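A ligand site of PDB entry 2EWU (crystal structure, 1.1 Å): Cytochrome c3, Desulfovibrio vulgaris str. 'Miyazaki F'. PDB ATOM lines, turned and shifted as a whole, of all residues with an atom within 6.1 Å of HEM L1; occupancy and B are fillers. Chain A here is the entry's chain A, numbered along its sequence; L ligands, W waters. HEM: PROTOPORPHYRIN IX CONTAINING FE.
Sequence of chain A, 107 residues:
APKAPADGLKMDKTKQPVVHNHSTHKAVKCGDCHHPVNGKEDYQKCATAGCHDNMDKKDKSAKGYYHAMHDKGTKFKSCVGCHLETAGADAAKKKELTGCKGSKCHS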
ATOM      1  N   MET A  11     -10.192  32.606  -6.614  1.00  0.00           N
ATOM      2  CA  MET A  11      -9.782  32.900  -5.268  1.00  0.00           C
ATOM      3  C   MET A  11      -8.269  33.032  -5.322  1.00  0.00           C
ATOM      4  O   MET A  11      -7.574  32.080  -5.687  1.00  0.00           O
ATOM      5  CB  MET A  11     -10.210  31.757  -4.337  1.00  0.00           C
ATOM      6  CG  MET A  11     -11.760  31.540  -4.369  1.00  0.00           C
ATOM      7  SD  MET A  11     -12.284  30.098  -3.430  1.00  0.00           S
ATOM      8  CE  MET A  11     -12.117  30.792  -1.744  1.00  0.00           C
ATOM      9  N   ASP A  12      -7.770  34.231  -4.996  1.00  0.00           N
ATOM     10  CA  ASP A  12      -6.391  34.561  -5.291  1.00  0.00           C
ATOM     11  C   ASP A  12      -5.675  35.302  -4.159  1.00  0.00           C
ATOM     12  O   ASP A  12      -4.791  36.119  -4.395  1.00  0.00           O
ATOM     13  CB  ASP A  12      -6.330  35.382  -6.603  1.00  0.00           C
ATOM     14  CG  ASP A  12      -7.127  36.668  -6.499  1.00  0.00           C
ATOM     15  OD1 ASP A  12      -7.529  37.074  -5.374  1.00  0.00           O
ATOM     16  OD2 ASP A  12      -7.348  37.283  -7.595  1.00  0.00           O
ATOM     17  N   LYS A  13      -6.031  34.905  -2.930  1.00  0.00           N
ATOM     18  CA  LYS A  13      -5.291  35.481  -1.786  1.00  0.00           C
ATOM     19  C   LYS A  13      -3.903  34.908  -1.601  1.00  0.00           C
ATOM     20  O   LYS A  13      -3.112  35.501  -0.836  1.00  0.00           O
ATOM     21  CB  LYS A  13      -6.059  35.223  -0.506  1.00  0.00           C
ATOM     22  CG  LYS A  13      -7.521  35.677  -0.511  1.00  0.00           C
ATOM     23  CD  LYS A  13      -7.812  37.058  -0.908  1.00  0.00           C
ATOM     24  CE  LYS A  13      -7.210  38.041   0.066  1.00  0.00           C
ATOM     25  NZ  LYS A  13      -7.718  39.408  -0.320  1.00  0.00           N
ATOM     26  N   THR A  14      -3.605  33.821  -2.248  1.00  0.00           N
ATOM     27  CA  THR A  14      -2.385  33.058  -2.054  1.00  0.00           C
ATOM     28  C   THR A  14      -1.651  32.814  -3.368  1.00  0.00           C
ATOM     29  O   THR A  14      -2.210  33.118  -4.452  1.00  0.00           O
ATOM     30  CB  THR A  14      -2.626  31.700  -1.379  1.00  0.00           C
ATOM     31  OG1 THR A  14      -3.075  30.733  -2.342  1.00  0.00           O
ATOM     32  CG2 THR A  14      -3.669  31.796  -0.239  1.00  0.00           C
ATOM     33  N   LYS A  15      -0.450  32.217  -3.310  1.00  0.00           N
ATOM     34  CA  LYS A  15       0.257  31.851  -4.545  1.00  0.00           C
ATOM     35  C   LYS A  15      -0.237  30.539  -5.127  1.00  0.00           C
ATOM     36  O   LYS A  15       0.333  30.059  -6.111  1.00  0.00           O
ATOM     37  CB  LYS A  15       1.778  31.783  -4.284  1.00  0.00           C
ATOM     38  CG  LYS A  15       2.323  33.191  -3.977  1.00  0.00           C
ATOM     39  CD  LYS A  15       3.823  33.111  -3.782  1.00  0.00           C
ATOM     40  CE  LYS A  15       4.298  34.458  -3.262  1.00  0.00           C
ATOM     41  NZ  LYS A  15       5.792  34.452  -3.094  1.00  0.00           N
ATOM     42  N   GLN A  16      -1.311  30.004  -4.559  1.00  0.00           N
ATOM     43  CA  GLN A  16      -1.899  28.792  -5.103  1.00  0.00           C
ATOM     44  C   GLN A  16      -3.379  29.066  -5.404  1.00  0.00           C
ATOM     45  O   GLN A  16      -4.274  28.516  -4.775  1.00  0.00           O
ATOM     46  CB  GLN A  16      -1.755  27.597  -4.138  1.00  0.00           C
ATOM     47  CG  GLN A  16      -0.340  27.373  -3.575  1.00  0.00           C
ATOM     48  CD  GLN A  16       0.748  27.179  -4.570  1.00  0.00           C
ATOM     49  OE1 GLN A  16       0.466  26.608  -5.625  1.00  0.00           O
ATOM     50  NE2 GLN A  16       1.945  27.612  -4.220  1.00  0.00           N
ATOM     51  N   PRO A  17      -3.655  29.958  -6.325  1.00  0.00           N
ATOM     52  CA  PRO A  17      -5.037  30.413  -6.529  1.00  0.00           C
ATOM     53  C   PRO A  17      -5.910  29.277  -7.080  1.00  0.00           C
ATOM     54  O   PRO A  17      -5.446  28.366  -7.775  1.00  0.00           O
ATOM     55  CB  PRO A  17      -4.912  31.523  -7.565  1.00  0.00           C
ATOM     56  CG  PRO A  17      -3.615  31.244  -8.263  1.00  0.00           C
ATOM     57  CD  PRO A  17      -2.730  30.672  -7.231  1.00  0.00           C
ATOM     58  N   VAL A  18      -7.229  29.395  -6.801  1.00  0.00           N
ATOM     59  CA  VAL A  18      -8.158  28.314  -7.143  1.00  0.00           C
ATOM     60  C   VAL A  18      -9.419  28.940  -7.745  1.00  0.00           C
ATOM     61  O   VAL A  18      -9.964  29.909  -7.235  1.00  0.00           O
ATOM     62  CB  VAL A  18      -8.551  27.503  -5.884  1.00  0.00           C
ATOM     63  CG1 VAL A  18      -9.658  26.474  -6.108  1.00  0.00           C
ATOM     64  CG2 VAL A  18      -7.317  26.798  -5.311  1.00  0.00           C
ATOM     65  N   MET A  55      -3.431  34.812   7.017  1.00  0.00           N
ATOM     66  CA  MET A  55      -2.815  34.108   5.926  1.00  0.00           C
ATOM     67  C   MET A  55      -1.660  33.209   6.350  1.00  0.00           C
ATOM     68  O   MET A  55      -0.885  32.794   5.506  1.00  0.00           O
ATOM     69  CB  MET A  55      -2.415  35.125   4.869  1.00  0.00           C
ATOM     70  CG  MET A  55      -3.607  35.815   4.208  1.00  0.00           C
ATOM     71  SD  MET A  55      -4.555  34.636   3.194  1.00  0.00           S
ATOM     72  CE  MET A  55      -6.177  35.392   3.289  1.00  0.00           C
ATOM     73  N   ASP A  56      -1.570  32.878   7.645  1.00  0.00           N
ATOM     74  CA  ASP A  56      -0.671  31.838   8.089  1.00  0.00           C
ATOM     75  C   ASP A  56      -1.385  30.486   7.940  1.00  0.00           C
ATOM     76  O   ASP A  56      -2.395  30.280   8.615  1.00  0.00           O
ATOM     77  CB  ASP A  56      -0.205  32.027   9.518  1.00  0.00           C
ATOM     78  CG  ASP A  56       0.818  30.932   9.853  1.00  0.00           C
ATOM     79  OD1 ASP A  56       0.497  29.791   9.979  1.00  0.00           O
ATOM     80  OD2 ASP A  56       2.066  31.185   9.917  1.00  0.00           O
ATOM     81  N   LYS A  57      -0.861  29.677   7.070  1.00  0.00           N
ATOM     82  CA  LYS A  57      -1.586  28.415   6.669  1.00  0.00           C
ATOM     83  C   LYS A  57      -1.582  27.411   7.794  1.00  0.00           C
ATOM     84  O   LYS A  57      -2.278  26.398   7.626  1.00  0.00           O
ATOM     85  CB  LYS A  57      -1.054  27.866   5.331  1.00  0.00           C
ATOM     86  CG  LYS A  57       0.374  27.309   5.425  1.00  0.00           C
ATOM     87  CD  LYS A  57       0.758  26.779   4.020  1.00  0.00           C
ATOM     88  CE  LYS A  57       2.267  26.380   4.053  1.00  0.00           C
ATOM     89  NZ  LYS A  57       2.662  25.856   2.707  1.00  0.00           N
ATOM     90  N   TYR A  65      -7.417  31.427   7.051  1.00  0.00           N
ATOM     91  CA  TYR A  65      -7.966  31.256   5.687  1.00  0.00           C
ATOM     92  C   TYR A  65      -7.740  29.829   5.170  1.00  0.00           C
ATOM     93  O   TYR A  65      -8.658  29.181   4.669  1.00  0.00           O
ATOM     94  CB  TYR A  65      -7.322  32.302   4.818  1.00  0.00           C
ATOM     95  CG  TYR A  65      -7.822  32.330   3.384  1.00  0.00           C
ATOM     96  CD1 TYR A  65      -7.007  31.875   2.343  1.00  0.00           C
ATOM     97  CD2 TYR A  65      -9.060  32.838   3.036  1.00  0.00           C
ATOM     98  CE1 TYR A  65      -7.444  31.922   1.028  1.00  0.00           C
ATOM     99  CE2 TYR A  65      -9.516  32.898   1.713  1.00  0.00           C
ATOM    100  CZ  TYR A  65      -8.672  32.424   0.709  1.00  0.00           C
ATOM    101  OH  TYR A  65      -9.101  32.465  -0.586  1.00  0.00           O
ATOM    102  N   TYR A  66      -6.508  29.324   5.253  1.00  0.00           N
ATOM    103  CA  TYR A  66      -6.202  27.979   4.806  1.00  0.00           C
ATOM    104  C   TYR A  66      -7.125  26.999   5.525  1.00  0.00           C
ATOM    105  O   TYR A  66      -7.676  26.068   4.924  1.00  0.00           O
ATOM    106  CB  TYR A  66      -4.715  27.641   5.060  1.00  0.00           C
ATOM    107  CG  TYR A  66      -4.332  26.233   4.625  1.00  0.00           C
ATOM    108  CD1 TYR A  66      -4.563  25.125   5.456  1.00  0.00           C
ATOM    109  CD2 TYR A  66      -3.732  25.994   3.376  1.00  0.00           C
ATOM    110  CE1 TYR A  66      -4.224  23.830   5.058  1.00  0.00           C
ATOM    111  CE2 TYR A  66      -3.372  24.720   2.962  1.00  0.00           C
ATOM    112  CZ  TYR A  66      -3.632  23.665   3.823  1.00  0.00           C
ATOM    113  OH  TYR A  66      -3.273  22.411   3.397  1.00  0.00           O
ATOM    114  N   MET A  69     -10.608  26.495   4.198  1.00  0.00           N
ATOM    115  CA  MET A  69     -10.746  25.844   2.921  1.00  0.00           C
ATOM    116  C   MET A  69     -10.370  24.375   2.923  1.00  0.00           C
ATOM    117  O   MET A  69     -10.784  23.636   2.033  1.00  0.00           O
ATOM    118  CB  MET A  69      -9.930  26.526   1.824  1.00  0.00           C
ATOM    119  CG  MET A  69     -10.132  28.053   1.764  1.00  0.00           C
ATOM    120  SD  MET A  69     -11.883  28.478   1.517  1.00  0.00           S
ATOM    121  CE  MET A  69     -11.794  30.216   1.924  1.00  0.00           C
ATOM    122  N   HIS A  70      -9.578  23.936   3.917  1.00  0.00           N
ATOM    123  CA  HIS A  70      -8.947  22.606   3.838  1.00  0.00           C
ATOM    124  C   HIS A  70      -9.299  21.635   4.953  1.00  0.00           C
ATOM    125  O   HIS A  70      -9.113  20.426   4.747  1.00  0.00           O
ATOM    126  CB  HIS A  70      -7.408  22.717   3.802  1.00  0.00           C
ATOM    127  CG  HIS A  70      -6.878  23.417   2.570  1.00  0.00           C
ATOM    128  ND1 HIS A  70      -6.785  24.807   2.542  1.00  0.00           N
ATOM    129  CD2 HIS A  70      -6.424  22.967   1.390  1.00  0.00           C
ATOM    130  CE1 HIS A  70      -6.327  25.142   1.341  1.00  0.00           C
ATOM    131  NE2 HIS A  70      -6.080  24.052   0.612  1.00  0.00           N
ATOM    132  N   CYS A  79     -14.095  23.333   1.808  1.00  0.00           N
ATOM    133  CA  CYS A  79     -14.001  22.800   0.457  1.00  0.00           C
ATOM    134  C   CYS A  79     -13.539  21.338   0.504  1.00  0.00           C
ATOM    135  O   CYS A  79     -14.162  20.441  -0.046  1.00  0.00           O
ATOM    136  CB  CYS A  79     -12.938  23.524  -0.363  1.00  0.00           C
ATOM    137  SG  CYS A  79     -12.931  25.337  -0.358  1.00  0.00           S
ATOM    138  N   VAL A  80     -12.395  21.090   1.159  1.00  0.00           N
ATOM    139  CA  VAL A  80     -11.850  19.722   1.170  1.00  0.00           C
ATOM    140  C   VAL A  80     -12.699  18.789   2.014  1.00  0.00           C
ATOM    141  O   VAL A  80     -12.914  17.621   1.612  1.00  0.00           O
ATOM    142  CB  VAL A  80     -10.377  19.735   1.677  1.00  0.00           C
ATOM    143  CG1 VAL A  80      -9.823  18.297   1.827  1.00  0.00           C
ATOM    144  CG2 VAL A  80      -9.492  20.506   0.711  1.00  0.00           C
ATOM    145  N   HIS A  83     -15.703  17.813   0.005  1.00  0.00           N
ATOM    146  CA  HIS A  83     -15.264  16.949  -1.099  1.00  0.00           C
ATOM    147  C   HIS A  83     -14.864  15.554  -0.650  1.00  0.00           C
ATOM    148  O   HIS A  83     -15.049  14.561  -1.351  1.00  0.00           O
ATOM    149  CB  HIS A  83     -14.093  17.603  -1.839  1.00  0.00           C
ATOM    150  CG  HIS A  83     -14.547  18.744  -2.692  1.00  0.00           C
ATOM    151  ND1 HIS A  83     -13.665  19.261  -3.642  1.00  0.00           N
ATOM    152  CD2 HIS A  83     -15.675  19.497  -2.800  1.00  0.00           C
ATOM    153  CE1 HIS A  83     -14.260  20.263  -4.260  1.00  0.00           C
ATOM    154  NE2 HIS A  83     -15.488  20.449  -3.790  1.00  0.00           N
ATOM    155  N   GLU A  96      -9.276  13.762  -7.765  1.00  0.00           N
ATOM    156  CA  GLU A  96      -9.843  14.898  -8.433  1.00  0.00           C
ATOM    157  C   GLU A  96     -10.336  16.009  -7.508  1.00  0.00           C
ATOM    158  O   GLU A  96     -10.181  17.203  -7.761  1.00  0.00           O
ATOM    159  CB  GLU A  96     -11.077  14.439  -9.244  1.00  0.00           C
ATOM    160  CG  GLU A  96     -10.732  13.661 -10.483  1.00  0.00           C
ATOM    161  CD  GLU A  96     -12.060  13.174 -11.069  1.00  0.00           C
ATOM    162  OE1 GLU A  96     -13.035  13.929 -11.246  1.00  0.00           O
ATOM    163  OE2 GLU A  96     -12.155  11.975 -11.398  1.00  0.00           O
ATOM    164  N   LEU A  97     -10.979  15.597  -6.388  1.00  0.00           N
ATOM    165  CA  LEU A  97     -11.704  16.554  -5.558  1.00  0.00           C
ATOM    166  C   LEU A  97     -10.929  16.939  -4.298  1.00  0.00           C
ATOM    167  O   LEU A  97     -11.230  17.957  -3.705  1.00  0.00           O
ATOM    168  CB  LEU A  97     -13.058  15.984  -5.150  1.00  0.00           C
ATOM    169  CG  LEU A  97     -14.002  15.698  -6.308  1.00  0.00           C
ATOM    170  CD1 LEU A  97     -15.284  15.066  -5.713  1.00  0.00           C
ATOM    171  CD2 LEU A  97     -14.299  16.958  -7.119  1.00  0.00           C
ATOM    172  N   THR A  98      -9.934  16.109  -3.893  1.00  0.00           N
ATOM    173  CA  THR A  98      -9.216  16.390  -2.653  1.00  0.00           C
ATOM    174  C   THR A  98      -7.707  16.363  -2.802  1.00  0.00           C
ATOM    175  O   THR A  98      -6.999  16.678  -1.829  1.00  0.00           O
ATOM    176  CB  THR A  98      -9.600  15.459  -1.496  1.00  0.00           C
ATOM    177  OG1 THR A  98      -9.151  14.119  -1.704  1.00  0.00           O
ATOM    178  CG2 THR A  98     -11.111  15.473  -1.334  1.00  0.00           C
ATOM    179  N   GLY A  99      -7.154  16.059  -3.995  1.00  0.00           N
ATOM    180  CA  GLY A  99      -5.696  15.942  -4.156  1.00  0.00           C
ATOM    181  C   GLY A  99      -5.068  17.298  -3.982  1.00  0.00           C
ATOM    182  O   GLY A  99      -5.588  18.340  -4.342  1.00  0.00           O
ATOM    183  N   CYS A 100      -3.854  17.269  -3.362  1.00  0.00           N
ATOM    184  CA  CYS A 100      -3.151  18.540  -3.131  1.00  0.00           C
ATOM    185  C   CYS A 100      -2.485  19.060  -4.379  1.00  0.00           C
ATOM    186  O   CYS A 100      -2.175  20.253  -4.446  1.00  0.00           O
ATOM    187  CB  CYS A 100      -2.089  18.317  -2.045  1.00  0.00           C
ATOM    188  SG  CYS A 100      -2.730  17.615  -0.517  1.00  0.00           S
ATOM    189  N   LYS A 101      -2.246  18.205  -5.356  1.00  0.00           N
ATOM    190  CA  LYS A 101      -1.752  18.621  -6.674  1.00  0.00           C
ATOM    191  C   LYS A 101      -2.478  17.723  -7.675  1.00  0.00           C
ATOM    192  O   LYS A 101      -2.982  16.677  -7.322  1.00  0.00           O
ATOM    193  CB  LYS A 101      -0.257  18.510  -6.863  1.00  0.00           C
ATOM    194  CG  LYS A 101       0.270  17.092  -6.689  1.00  0.00           C
ATOM    195  CD  LYS A 101       1.810  17.169  -6.835  1.00  0.00           C
ATOM    196  CE  LYS A 101       2.374  15.772  -7.048  1.00  0.00           C
ATOM    197  NZ  LYS A 101       2.140  15.263  -8.404  1.00  0.00           N
ATOM    198  N   SER A 103      -5.244  18.106  -8.999  1.00  0.00           N
ATOM    199  CA  SER A 103      -6.691  17.988  -8.672  1.00  0.00           C
ATOM    200  C   SER A 103      -7.450  19.077  -9.392  1.00  0.00           C
ATOM    201  O   SER A 103      -6.868  19.911 -10.075  1.00  0.00           O
ATOM    202  CB  SER A 103      -6.921  18.085  -7.179  1.00  0.00           C
ATOM    203  OG  SER A 103      -6.621  19.404  -6.696  1.00  0.00           O
ATOM    204  N   LYS A 104      -8.788  19.141  -9.207  1.00  0.00           N
ATOM    205  CA  LYS A 104      -9.573  20.198  -9.806  1.00  0.00           C
ATOM    206  C   LYS A 104      -9.348  21.530  -9.086  1.00  0.00           C
ATOM    207  O   LYS A 104      -9.734  22.554  -9.632  1.00  0.00           O
ATOM    208  CB  LYS A 104     -11.033  19.824  -9.860  1.00  0.00           C
ATOM    209  CG  LYS A 104     -11.283  18.663 -10.838  1.00  0.00           C
ATOM    210  CD  LYS A 104     -12.696  18.317 -11.169  1.00  0.00           C
ATOM    211  CE  LYS A 104     -12.647  17.259 -12.304  1.00  0.00           C
ATOM    212  NZ  LYS A 104     -12.442  17.938 -13.617  1.00  0.00           N
ATOM    213  N   CYS A 105      -8.771  21.523  -7.913  1.00  0.00           N
ATOM    214  CA  CYS A 105      -8.433  22.787  -7.227  1.00  0.00           C
ATOM    215  C   CYS A 105      -7.029  23.260  -7.562  1.00  0.00           C
ATOM    216  O   CYS A 105      -6.834  24.438  -7.862  1.00  0.00           O
ATOM    217  CB  CYS A 105      -8.575  22.671  -5.728  1.00  0.00           C
ATOM    218  SG  CYS A 105     -10.272  22.229  -5.281  1.00  0.00           S
ATOM    219  N   HIS A 106      -6.032  22.358  -7.487  1.00  0.00           N
ATOM    220  CA  HIS A 106      -4.640  22.740  -7.667  1.00  0.00           C
ATOM    221  C   HIS A 106      -3.994  21.895  -8.760  1.00  0.00           C
ATOM    222  O   HIS A 106      -3.999  20.692  -8.655  1.00  0.00           O
ATOM    223  CB  HIS A 106      -3.852  22.481  -6.374  1.00  0.00           C
ATOM    224  CG  HIS A 106      -4.243  23.314  -5.173  1.00  0.00           C
ATOM    225  ND1 HIS A 106      -4.279  24.666  -5.153  1.00  0.00           N
ATOM    226  CD2 HIS A 106      -4.605  22.913  -3.932  1.00  0.00           C
ATOM    227  CE1 HIS A 106      -4.625  25.079  -3.917  1.00  0.00           C
ATOM    228  NE2 HIS A 106      -4.845  24.041  -3.146  1.00  0.00           N
HETATM  229  CHA HEM L   1      -4.709  27.409  -1.108  1.00  0.00           C
HETATM  230  CHB HEM L   1      -2.309  23.326  -0.163  1.00  0.00           C
HETATM  231  CHC HEM L   1      -6.076  20.692  -1.534  1.00  0.00           C
HETATM  232  CHD HEM L   1      -8.587  24.772  -2.183  1.00  0.00           C
HETATM  233  C1A HEM L   1      -3.670  26.520  -0.827  1.00  0.00           C
HETATM  234  C2A HEM L   1      -2.347  26.879  -0.472  1.00  0.00           C
HETATM  235  C3A HEM L   1      -1.646  25.721  -0.245  1.00  0.00           C
HETATM  236  C4A HEM L   1      -2.574  24.676  -0.458  1.00  0.00           C
HETATM  237  CMA HEM L   1      -0.215  25.525   0.200  1.00  0.00           C
HETATM  238  CAA HEM L   1      -1.815  28.301  -0.287  1.00  0.00           C
HETATM  239  CBA HEM L   1      -1.771  28.691   1.177  1.00  0.00           C
HETATM  240  CGA HEM L   1      -0.949  29.929   1.421  1.00  0.00           C
HETATM  241  O1A HEM L   1       0.192  30.012   0.918  1.00  0.00           O
HETATM  242  O2A HEM L   1      -1.452  30.865   2.049  1.00  0.00           O
HETATM  243  C1B HEM L   1      -3.199  22.236  -0.256  1.00  0.00           C
HETATM  244  C2B HEM L   1      -2.874  20.926   0.086  1.00  0.00           C
HETATM  245  C3B HEM L   1      -3.948  20.140  -0.342  1.00  0.00           C
HETATM  246  C4B HEM L   1      -4.872  21.045  -0.921  1.00  0.00           C
HETATM  247  CMB HEM L   1      -1.600  20.496   0.798  1.00  0.00           C
HETATM  248  CAB HEM L   1      -4.180  18.722  -0.143  1.00  0.00           C
HETATM  249  CBB HEM L   1      -4.598  18.364   1.237  1.00  0.00           C
HETATM  250  C1C HEM L   1      -7.061  21.614  -2.002  1.00  0.00           C
HETATM  251  C2C HEM L   1      -8.214  21.228  -2.702  1.00  0.00           C
HETATM  252  C3C HEM L   1      -8.996  22.373  -2.821  1.00  0.00           C
HETATM  253  C4C HEM L   1      -8.216  23.421  -2.264  1.00  0.00           C
HETATM  254  CMC HEM L   1      -8.522  19.817  -3.164  1.00  0.00           C
HETATM  255  CAC HEM L   1     -10.322  22.526  -3.433  1.00  0.00           C
HETATM  256  CBC HEM L   1     -11.390  21.584  -2.927  1.00  0.00           C
HETATM  257  C1D HEM L   1      -7.795  25.834  -1.793  1.00  0.00           C
HETATM  258  C2D HEM L   1      -8.218  27.160  -1.792  1.00  0.00           C
HETATM  259  C3D HEM L   1      -7.097  27.931  -1.535  1.00  0.00           C
HETATM  260  C4D HEM L   1      -6.034  27.039  -1.401  1.00  0.00           C
HETATM  261  CMD HEM L   1      -9.640  27.661  -2.025  1.00  0.00           C
HETATM  262  CAD HEM L   1      -7.011  29.462  -1.504  1.00  0.00           C
HETATM  263  CBD HEM L   1      -6.807  30.050  -2.910  1.00  0.00           C
HETATM  264  CGD HEM L   1      -6.420  31.523  -2.867  1.00  0.00           C
HETATM  265  O1D HEM L   1      -7.207  32.346  -2.329  1.00  0.00           O
HETATM  266  O2D HEM L   1      -5.300  31.849  -3.360  1.00  0.00           O
HETATM  267  NA  HEM L   1      -3.800  25.168  -0.786  1.00  0.00           N
HETATM  268  NB  HEM L   1      -4.402  22.303  -0.851  1.00  0.00           N
HETATM  269  NC  HEM L   1      -7.019  22.951  -1.821  1.00  0.00           N
HETATM  270  ND  HEM L   1      -6.470  25.773  -1.538  1.00  0.00           N
HETATM  271 FE   HEM L   1      -5.417  24.051  -1.255  1.00  0.00          FE
HETATM  272  CHA HEM L   2     -17.059  20.037  -7.293  1.00  0.00           C
HETATM  273  CHB HEM L   2     -14.106  23.497  -5.746  1.00  0.00           C
HETATM  274  CHC HEM L   2     -16.585  23.740  -1.642  1.00  0.00           C
HETATM  275  CHD HEM L   2     -19.310  20.046  -3.012  1.00  0.00           C
HETATM  276  C1A HEM L   2     -16.040  20.999  -7.241  1.00  0.00           C
HETATM  277  C2A HEM L   2     -15.114  21.225  -8.291  1.00  0.00           C
HETATM  278  C3A HEM L   2     -14.250  22.189  -7.833  1.00  0.00           C
HETATM  279  C4A HEM L   2     -14.723  22.543  -6.578  1.00  0.00           C
HETATM  280  CMA HEM L   2     -13.058  22.821  -8.524  1.00  0.00           C
HETATM  281  CAA HEM L   2     -15.083  20.497  -9.621  1.00  0.00           C
HETATM  282  CBA HEM L   2     -16.119  21.121 -10.621  1.00  0.00           C
HETATM  283  CGA HEM L   2     -15.698  22.559 -10.938  1.00  0.00           C
HETATM  284  O1A HEM L   2     -14.656  22.713 -11.624  1.00  0.00           O
HETATM  285  O2A HEM L   2     -16.406  23.483 -10.537  1.00  0.00           O
HETATM  286  C1B HEM L   2     -14.522  23.890  -4.465  1.00  0.00           C
HETATM  287  C2B HEM L   2     -13.895  24.893  -3.682  1.00  0.00           C
HETATM  288  C3B HEM L   2     -14.610  24.978  -2.508  1.00  0.00           C
HETATM  289  C4B HEM L   2     -15.648  24.005  -2.617  1.00  0.00           C
HETATM  290  CMB HEM L   2     -12.665  25.680  -4.140  1.00  0.00           C
HETATM  291  CAB HEM L   2     -14.433  25.854  -1.343  1.00  0.00           C
HETATM  292  CBB HEM L   2     -14.306  27.321  -1.610  1.00  0.00           C
HETATM  293  C1C HEM L   2     -17.500  22.673  -1.601  1.00  0.00           C
HETATM  294  C2C HEM L   2     -18.313  22.369  -0.461  1.00  0.00           C
HETATM  295  C3C HEM L   2     -19.125  21.320  -0.869  1.00  0.00           C
HETATM  296  C4C HEM L   2     -18.732  21.027  -2.197  1.00  0.00           C
HETATM  297  CMC HEM L   2     -18.210  23.159   0.839  1.00  0.00           C
HETATM  298  CAC HEM L   2     -20.119  20.572  -0.089  1.00  0.00           C
HETATM  299  CBC HEM L   2     -20.775  21.215   1.098  1.00  0.00           C
HETATM  300  C1D HEM L   2     -18.959  19.723  -4.340  1.00  0.00           C
HETATM  301  C2D HEM L   2     -19.608  18.743  -5.122  1.00  0.00           C
HETATM  302  C3D HEM L   2     -18.968  18.754  -6.333  1.00  0.00           C
HETATM  303  C4D HEM L   2     -17.975  19.716  -6.245  1.00  0.00           C
HETATM  304  CMD HEM L   2     -20.765  17.868  -4.668  1.00  0.00           C
HETATM  305  CAD HEM L   2     -19.215  17.844  -7.522  1.00  0.00           C
HETATM  306  CBD HEM L   2     -18.308  16.646  -7.461  1.00  0.00           C
HETATM  307  CGD HEM L   2     -18.080  15.956  -8.790  1.00  0.00           C
HETATM  308  O1D HEM L   2     -17.664  14.805  -8.706  1.00  0.00           O
HETATM  309  O2D HEM L   2     -18.615  16.260  -9.868  1.00  0.00           O
HETATM  310  NA  HEM L   2     -15.789  21.798  -6.204  1.00  0.00           N
HETATM  311  NB  HEM L   2     -15.550  23.356  -3.793  1.00  0.00           N
HETATM  312  NC  HEM L   2     -17.740  21.825  -2.593  1.00  0.00           N
HETATM  313  ND  HEM L   2     -17.991  20.316  -5.058  1.00  0.00           N
HETATM  314 FE   HEM L   2     -16.780  21.832  -4.424  1.00  0.00          FE
HETATM  315  O   HOH W   1       2.179  28.181   0.981  1.00  0.00           O
HETATM  316  O   HOH W   2      -0.621  33.232   2.787  1.00  0.00           O
HETATM  317  O   HOH W   3      -3.704  31.341   3.492  1.00  0.00           O
HETATM  318  O   HOH W   4       0.979  31.848  -0.825  1.00  0.00           O
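The backbone NH of Asp 12 lies within hydrogen-bond range of an oxygen (O1D) of HEM L1, 3.3 Å away. The side-chain sulfur (SG) of Cys 105 is bonded to a carbon (CAC) of HEM L1, 1.9 Å away. An oxygen (O2D) of HEM L1 is in hydrogen-bond range of the side-chain hydroxyl of Thr 14. A ring nitrogen (NE2) of His 83 binds an iron atom (FE) of HEM L2. A ring nitrogen (NE2) of His 70 binds an iron atom (FE) of HEM L1, 2.0 Å away. The backbone NH (N) of Lys 13 is in hydrogen-bond range of an oxygen (O1D) of HEM L1 (2.9 Å). CAB of HEM L2 is bonded to SG of Cys 79. An iron atom (FE) of HEM L1 is bound by a ring nitrogen (NE2) of His 106 (2.0 Å). OH of Tyr 65 lies within hydrogen-bond range of O1D of HEM L1, at 2.6 Å. The backbone NH (N) of Thr 14 lies within hydrogen-bond range of an oxygen (O2D) of HEM L1 (2.8 Å). A carbon (CAB) of HEM L1 is bonded to the side-chain sulfur (SG) of Cys 100 (1.9 Å).
The backbone carbonyl oxygen of Val 18 sits at hydrogen-bond distance from the backbone NH of Met 11 (2.8 Å). The backbone NH of Cys 79 lies close to the backbone carbonyl oxygen of Met 69, at 3.3 Å. N of His 106 sits at hydrogen-bond distance from OG of Ser 103 (3.1 Å). OG1 of Thr 14 is in hydrogen-bond range of N of Gln 16, 2.9 Å away. OG of Ser 103 is in hydrogen-bond range of O of Gly 99 (2.8 Å). The backbone carbonyl oxygen (O) of Tyr 66 sits at hydrogen-bond distance from a ring nitrogen (ND1) of His 70, at 2.8 Å. The backbone carbonyl oxygen (O) of Met 69 sits at hydrogen-bond distance from the backbone NH (N) of Val 80, at 3.1 Å. The backbone NH (N) of Cys 105 sits close to the side-chain hydroxyl (OG) of Ser 103 (3.3 Å).
O of Met 11 lies close to O2D of HEM L1, 3.3 Å away. O of Gln 16 touches CBD of HEM L1 (3.5 Å). Pro 17 touches HEM L1 (CA to O2D, 3.5 Å). CG2 of Val 18 touches C2D of HEM L1, at 3.7 Å. O of Met 55 touches O2A of HEM L1 (3.999 Å). NZ of Lys 57 touches CMA of HEM L1, at 3.8 Å. Tyr 66 touches HEM L1 (CE2 to C4A, 3.5 Å). Met 69 touches HEM L1 (CG to CMD, 3.8 Å). Cys 79 touches HEM L1 (CB to CBC, 3.6 Å). Val 80 touches HEM L1. His 83 touches HEM L1 (ND1 to CBC, 3.3 Å). Leu 97 touches HEM L1 (O to CMC, 3.3 Å). Thr 98 touches HEM L1 (CA to CMC, 3.5 Å). O of Gly 99 touches CMC of HEM L1, at 3.5 Å. Hydrophobic or aromatic side chains within 4 Å of HEM L1: Met 11, Val 18, Tyr 65, Tyr 66, Met 69, His 70, Val 80, His 83 and His 106. Of the 28 residues printed, 22 come within 4 Å of HEM L1.
Water W2 bridges O2A of HEM L1 and O of Met 55. Water W4 lies within hydrogen-bond range of O1A of HEM L1 (2.7 Å) and N of Lys 15 (2.9 Å). Water W1 bridges O1A of HEM L1 (2.7 Å) and NZ of Lys 57 (2.9 Å). Water W3 lies within hydrogen-bond range of O2A of HEM L1 (2.7 Å) and SD of Met 55 (3.4 Å).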
